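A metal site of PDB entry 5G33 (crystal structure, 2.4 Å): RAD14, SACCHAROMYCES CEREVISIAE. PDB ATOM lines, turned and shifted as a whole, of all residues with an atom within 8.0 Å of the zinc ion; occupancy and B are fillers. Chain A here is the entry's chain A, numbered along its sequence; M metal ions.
The side-chain sulfur (SG) of Cys 27 lies close to the backbone NH (N) of Gln 29, 3.7 Å away. The backbone NH (N) of Asn 11 lies close to the side-chain sulfur (SG) of Cys 8. The backbone NH of Ile 10 sits close to the side-chain sulfur of Cys 8, 3.4 Å away. O of Asn 11 sits at hydrogen-bond distance from N of Cys 5, 2.9 Å away. The side-chain sulfur (SG) of Cys 5 sits close to the backbone NH (N) of Glu 7 (3.7 Å). SG of Cys 27 sits close to ND2 of Asn 11, 3.5 Å away.
The zinc ion is bound by SG of Cys 5 (1.9 Å). SG of Cys 30 is bound to the zinc ion (2.1 Å). The side-chain sulfur (SG) of Cys 8 binds the zinc ion (2.5 Å). The side-chain sulfur (SG) of Cys 27 is bound to the zinc ion (2.7 Å). The zinc ion has four donor atoms within binding distance.
Of the 21 residues printed, 4 come within 4 Å of the zinc ion. The nearest printed residue that does not touch the zinc ion is Glu 7 (4.3 Å).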
ATOM      1  N   LYS A   4     -19.707  24.335 -31.813  1.00  0.00           N
ATOM      2  CA  LYS A   4     -18.457  23.995 -31.145  1.00  0.00           C
ATOM      3  C   LYS A   4     -17.249  24.670 -31.754  1.00  0.00           C
ATOM      4  O   LYS A   4     -17.135  24.715 -32.976  1.00  0.00           O
ATOM      5  CB  LYS A   4     -18.221  22.486 -31.238  1.00  0.00           C
ATOM      6  CG  LYS A   4     -19.298  21.656 -30.580  1.00  0.00           C
ATOM      7  CD  LYS A   4     -19.173  21.653 -29.061  1.00  0.00           C
ATOM      8  CE  LYS A   4     -20.369  20.951 -28.396  1.00  0.00           C
ATOM      9  NZ  LYS A   4     -20.140  19.563 -27.902  1.00  0.00           N
ATOM     10  N   CYS A   5     -16.331  25.108 -30.919  1.00  0.00           N
ATOM     11  CA  CYS A   5     -15.023  25.598 -31.386  1.00  0.00           C
ATOM     12  C   CYS A   5     -14.449  24.623 -32.426  1.00  0.00           C
ATOM     13  O   CYS A   5     -14.313  23.429 -32.186  1.00  0.00           O
ATOM     14  CB  CYS A   5     -14.096  25.844 -30.171  1.00  0.00           C
ATOM     15  SG  CYS A   5     -12.327  25.945 -30.417  1.00  0.00           S
ATOM     16  N   ILE A   6     -14.171  25.165 -33.613  1.00  0.00           N
ATOM     17  CA  ILE A   6     -13.688  24.404 -34.782  1.00  0.00           C
ATOM     18  C   ILE A   6     -12.240  23.947 -34.713  1.00  0.00           C
ATOM     19  O   ILE A   6     -11.755  23.405 -35.685  1.00  0.00           O
ATOM     20  CB  ILE A   6     -13.793  25.254 -36.078  1.00  0.00           C
ATOM     21  CG1 ILE A   6     -12.738  26.397 -36.050  1.00  0.00           C
ATOM     22  CG2 ILE A   6     -15.212  25.776 -36.292  1.00  0.00           C
ATOM     23  CD1 ILE A   6     -13.084  27.646 -36.828  1.00  0.00           C
ATOM     24  N   GLU A   7     -11.528  24.252 -33.635  1.00  0.00           N
ATOM     25  CA  GLU A   7     -10.108  23.877 -33.479  1.00  0.00           C
ATOM     26  C   GLU A   7     -10.086  22.641 -32.593  1.00  0.00           C
ATOM     27  O   GLU A   7      -9.602  21.589 -32.991  1.00  0.00           O
ATOM     28  CB  GLU A   7      -9.361  25.092 -32.849  1.00  0.00           C
ATOM     29  CG  GLU A   7      -7.853  25.210 -33.079  1.00  0.00           C
ATOM     30  CD  GLU A   7      -7.406  25.361 -34.549  1.00  0.00           C
ATOM     31  OE1 GLU A   7      -8.052  26.125 -35.323  1.00  0.00           O
ATOM     32  OE2 GLU A   7      -6.386  24.743 -34.930  1.00  0.00           O
ATOM     33  N   CYS A   8     -10.706  22.741 -31.429  1.00  0.00           N
ATOM     34  CA  CYS A   8     -10.677  21.725 -30.436  1.00  0.00           C
ATOM     35  C   CYS A   8     -11.919  20.795 -30.404  1.00  0.00           C
ATOM     36  O   CYS A   8     -11.894  19.731 -29.762  1.00  0.00           O
ATOM     37  CB  CYS A   8     -10.542  22.406 -29.090  1.00  0.00           C
ATOM     38  SG  CYS A   8     -12.042  23.232 -28.578  1.00  0.00           S
ATOM     39  N   HIS A   9     -13.024  21.232 -31.008  1.00  0.00           N
ATOM     40  CA  HIS A   9     -14.292  20.492 -31.043  1.00  0.00           C
ATOM     41  C   HIS A   9     -15.001  20.295 -29.708  1.00  0.00           C
ATOM     42  O   HIS A   9     -16.051  19.654 -29.663  1.00  0.00           O
ATOM     43  CB  HIS A   9     -14.122  19.189 -31.825  1.00  0.00           C
ATOM     44  CG  HIS A   9     -13.435  19.391 -33.139  1.00  0.00           C
ATOM     45  ND1 HIS A   9     -13.828  20.352 -34.046  1.00  0.00           N
ATOM     46  CD2 HIS A   9     -12.352  18.780 -33.693  1.00  0.00           C
ATOM     47  CE1 HIS A   9     -13.036  20.329 -35.094  1.00  0.00           C
ATOM     48  NE2 HIS A   9     -12.141  19.379 -34.915  1.00  0.00           N
ATOM     49  N   ILE A  10     -14.514  20.963 -28.662  1.00  0.00           N
ATOM     50  CA  ILE A  10     -15.028  20.853 -27.292  1.00  0.00           C
ATOM     51  C   ILE A  10     -15.808  22.055 -26.792  1.00  0.00           C
ATOM     52  O   ILE A  10     -16.908  21.914 -26.289  1.00  0.00           O
ATOM     53  CB  ILE A  10     -13.857  20.671 -26.313  1.00  0.00           C
ATOM     54  CG1 ILE A  10     -13.072  19.374 -26.611  1.00  0.00           C
ATOM     55  CG2 ILE A  10     -14.350  20.646 -24.864  1.00  0.00           C
ATOM     56  CD1 ILE A  10     -11.589  19.530 -26.297  1.00  0.00           C
ATOM     57  N   ASN A  11     -15.197  23.251 -26.866  1.00  0.00           N
ATOM     58  CA  ASN A  11     -15.709  24.433 -26.170  1.00  0.00           C
ATOM     59  C   ASN A  11     -16.954  24.928 -26.905  1.00  0.00           C
ATOM     60  O   ASN A  11     -17.068  24.752 -28.125  1.00  0.00           O
ATOM     61  CB  ASN A  11     -14.620  25.496 -25.950  1.00  0.00           C
ATOM     62  CG  ASN A  11     -14.018  25.470 -24.524  1.00  0.00           C
ATOM     63  OD1 ASN A  11     -14.699  25.201 -23.519  1.00  0.00           O
ATOM     64  ND2 ASN A  11     -12.741  25.839 -24.425  1.00  0.00           N
ATOM     65  N   ILE A  12     -17.929  25.439 -26.150  1.00  0.00           N
ATOM     66  CA  ILE A  12     -19.095  26.097 -26.753  1.00  0.00           C
ATOM     67  C   ILE A  12     -19.073  27.637 -26.581  1.00  0.00           C
ATOM     68  O   ILE A  12     -19.981  28.298 -27.090  1.00  0.00           O
ATOM     69  CB  ILE A  12     -20.448  25.588 -26.227  1.00  0.00           C
ATOM     70  CG1 ILE A  12     -20.454  25.511 -24.711  1.00  0.00           C
ATOM     71  CG2 ILE A  12     -20.807  24.267 -26.870  1.00  0.00           C
ATOM     72  CD1 ILE A  12     -21.830  25.669 -24.119  1.00  0.00           C
ATOM     73  N   GLU A  13     -18.084  28.188 -25.875  1.00  0.00           N
ATOM     74  CA  GLU A  13     -18.071  29.636 -25.602  1.00  0.00           C
ATOM     75  C   GLU A  13     -16.922  30.256 -26.360  1.00  0.00           C
ATOM     76  O   GLU A  13     -15.734  30.057 -26.048  1.00  0.00           O
ATOM     77  CB  GLU A  13     -18.165  29.975 -24.107  1.00  0.00           C
ATOM     78  CG  GLU A  13     -19.434  29.337 -23.527  1.00  0.00           C
ATOM     79  CD  GLU A  13     -19.794  29.787 -22.115  1.00  0.00           C
ATOM     80  OE1 GLU A  13     -19.514  30.981 -21.783  1.00  0.00           O
ATOM     81  OE2 GLU A  13     -20.346  28.946 -21.329  1.00  0.00           O
ATOM     82  N   MET A  14     -17.316  30.941 -27.432  1.00  0.00           N
ATOM     83  CA  MET A  14     -16.373  31.502 -28.386  1.00  0.00           C
ATOM     84  C   MET A  14     -15.713  32.766 -27.799  1.00  0.00           C
ATOM     85  O   MET A  14     -16.233  33.359 -26.877  1.00  0.00           O
ATOM     86  CB  MET A  14     -17.080  31.782 -29.725  1.00  0.00           C
ATOM     87  CG  MET A  14     -17.862  30.627 -30.303  1.00  0.00           C
ATOM     88  SD  MET A  14     -16.827  29.149 -30.402  1.00  0.00           S
ATOM     89  CE  MET A  14     -18.051  27.834 -30.587  1.00  0.00           C
ATOM     90  N   GLN A  25     -15.659  30.914 -35.415  1.00  0.00           N
ATOM     91  CA  GLN A  25     -16.138  30.070 -34.289  1.00  0.00           C
ATOM     92  C   GLN A  25     -14.928  29.420 -33.641  1.00  0.00           C
ATOM     93  O   GLN A  25     -14.692  28.219 -33.805  1.00  0.00           O
ATOM     94  CB  GLN A  25     -17.070  28.915 -34.743  1.00  0.00           C
ATOM     95  CG  GLN A  25     -18.431  29.265 -35.357  1.00  0.00           C
ATOM     96  CD  GLN A  25     -19.099  30.474 -34.706  1.00  0.00           C
ATOM     97  OE1 GLN A  25     -19.643  30.388 -33.586  1.00  0.00           O
ATOM     98  NE2 GLN A  25     -19.067  31.606 -35.419  1.00  0.00           N
ATOM     99  N   VAL A  26     -14.159  30.225 -32.911  1.00  0.00           N
ATOM    100  CA  VAL A  26     -12.956  29.813 -32.211  1.00  0.00           C
ATOM    101  C   VAL A  26     -13.024  30.297 -30.760  1.00  0.00           C
ATOM    102  O   VAL A  26     -13.336  31.477 -30.484  1.00  0.00           O
ATOM    103  CB  VAL A  26     -11.741  30.434 -32.842  1.00  0.00           C
ATOM    104  CG1 VAL A  26     -10.454  30.012 -32.129  1.00  0.00           C
ATOM    105  CG2 VAL A  26     -11.683  30.071 -34.317  1.00  0.00           C
ATOM    106  N   CYS A  27     -12.738  29.392 -29.839  1.00  0.00           N
ATOM    107  CA  CYS A  27     -12.777  29.735 -28.442  1.00  0.00           C
ATOM    108  C   CYS A  27     -11.437  30.420 -28.095  1.00  0.00           C
ATOM    109  O   CYS A  27     -10.553  30.483 -28.922  1.00  0.00           O
ATOM    110  CB  CYS A  27     -13.018  28.502 -27.597  1.00  0.00           C
ATOM    111  SG  CYS A  27     -11.500  27.624 -27.228  1.00  0.00           S
ATOM    112  N   LYS A  28     -11.343  30.914 -26.868  1.00  0.00           N
ATOM    113  CA  LYS A  28     -10.249  31.721 -26.432  1.00  0.00           C
ATOM    114  C   LYS A  28      -9.007  30.892 -26.301  1.00  0.00           C
ATOM    115  O   LYS A  28      -7.998  31.244 -26.852  1.00  0.00           O
ATOM    116  CB  LYS A  28     -10.585  32.365 -25.072  1.00  0.00           C
ATOM    117  CG  LYS A  28      -9.478  33.227 -24.443  1.00  0.00           C
ATOM    118  CD  LYS A  28      -9.626  34.697 -24.801  1.00  0.00           C
ATOM    119  CE  LYS A  28      -8.886  35.606 -23.839  1.00  0.00           C
ATOM    120  NZ  LYS A  28      -9.398  37.016 -23.927  1.00  0.00           N
ATOM    121  N   GLN A  29      -9.066  29.807 -25.552  1.00  0.00           N
ATOM    122  CA  GLN A  29      -7.898  28.899 -25.403  1.00  0.00           C
ATOM    123  C   GLN A  29      -7.212  28.464 -26.697  1.00  0.00           C
ATOM    124  O   GLN A  29      -5.994  28.404 -26.747  1.00  0.00           O
ATOM    125  CB  GLN A  29      -8.333  27.675 -24.642  1.00  0.00           C
ATOM    126  CG  GLN A  29      -7.255  26.590 -24.446  1.00  0.00           C
ATOM    127  CD  GLN A  29      -7.570  25.741 -23.242  1.00  0.00           C
ATOM    128  OE1 GLN A  29      -8.693  25.678 -22.809  1.00  0.00           O
ATOM    129  NE2 GLN A  29      -6.562  25.142 -22.676  1.00  0.00           N
ATOM    130  N   CYS A  30      -7.988  28.173 -27.719  1.00  0.00           N
ATOM    131  CA  CYS A  30      -7.433  27.747 -29.005  1.00  0.00           C
ATOM    132  C   CYS A  30      -6.874  28.931 -29.807  1.00  0.00           C
ATOM    133  O   CYS A  30      -6.028  28.730 -30.694  1.00  0.00           O
ATOM    134  CB  CYS A  30      -8.501  26.996 -29.827  1.00  0.00           C
ATOM    135  SG  CYS A  30      -9.050  25.407 -29.128  1.00  0.00           S
ATOM    136  N   SER A  31      -7.349  30.144 -29.522  1.00  0.00           N
ATOM    137  CA  SER A  31      -6.768  31.360 -30.133  1.00  0.00           C
ATOM    138  C   SER A  31      -5.327  31.535 -29.661  1.00  0.00           C
ATOM    139  O   SER A  31      -4.419  31.778 -30.480  1.00  0.00           O
ATOM    140  CB  SER A  31      -7.607  32.624 -29.848  1.00  0.00           C
ATOM    141  OG  SER A  31      -7.623  32.962 -28.472  1.00  0.00           O
ATOM    142  N   GLU A  33      -3.479  29.047 -28.500  1.00  0.00           N
ATOM    143  CA  GLU A  33      -2.668  27.859 -28.767  1.00  0.00           C
ATOM    144  C   GLU A  33      -2.313  27.789 -30.252  1.00  0.00           C
ATOM    145  O   GLU A  33      -1.541  26.947 -30.699  1.00  0.00           O
ATOM    146  CB  GLU A  33      -3.384  26.615 -28.225  1.00  0.00           C
ATOM    147  CG  GLU A  33      -3.422  26.646 -26.697  1.00  0.00           C
ATOM    148  CD  GLU A  33      -4.190  25.483 -25.990  1.00  0.00           C
ATOM    149  OE1 GLU A  33      -5.140  24.886 -26.587  1.00  0.00           O
ATOM    150  OE2 GLU A  33      -3.879  25.195 -24.785  1.00  0.00           O
ATOM    151  N   HIS A  34      -2.893  28.675 -31.043  1.00  0.00           N
ATOM    152  CA  HIS A  34      -2.631  28.703 -32.469  1.00  0.00           C
ATOM    153  C   HIS A  34      -2.534  30.182 -32.914  1.00  0.00           C
ATOM    154  O   HIS A  34      -3.444  30.669 -33.569  1.00  0.00           O
ATOM    155  CB  HIS A  34      -3.764  27.996 -33.229  1.00  0.00           C
ATOM    156  CG  HIS A  34      -3.885  26.529 -32.926  1.00  0.00           C
ATOM    157  ND1 HIS A  34      -3.499  25.551 -33.814  1.00  0.00           N
ATOM    158  CD2 HIS A  34      -4.371  25.886 -31.836  1.00  0.00           C
ATOM    159  CE1 HIS A  34      -3.741  24.372 -33.288  1.00  0.00           C
ATOM    160  NE2 HIS A  34      -4.262  24.554 -32.083  1.00  0.00           N
ATOM    161  N   TYR A  38      -4.516  33.017 -35.377  1.00  0.00           N
ATOM    162  CA  TYR A  38      -5.545  33.814 -34.684  1.00  0.00           C
ATOM    163  C   TYR A  38      -5.032  35.115 -34.011  1.00  0.00           C
ATOM    164  O   TYR A  38      -5.764  35.830 -33.328  1.00  0.00           O
ATOM    165  CB  TYR A  38      -6.255  32.910 -33.687  1.00  0.00           C
ATOM    166  CG  TYR A  38      -6.983  31.761 -34.340  1.00  0.00           C
ATOM    167  CD1 TYR A  38      -8.019  31.984 -35.206  1.00  0.00           C
ATOM    168  CD2 TYR A  38      -6.620  30.445 -34.095  1.00  0.00           C
ATOM    169  CE1 TYR A  38      -8.675  30.940 -35.825  1.00  0.00           C
ATOM    170  CE2 TYR A  38      -7.270  29.361 -34.693  1.00  0.00           C
ATOM    171  CZ  TYR A  38      -8.321  29.607 -35.548  1.00  0.00           C
ATOM    172  OH  TYR A  38      -8.973  28.564 -36.154  1.00  0.00           O
HETATM  173 ZN    ZN M   1     -11.149  25.578 -28.967  1.00  0.00          ZN
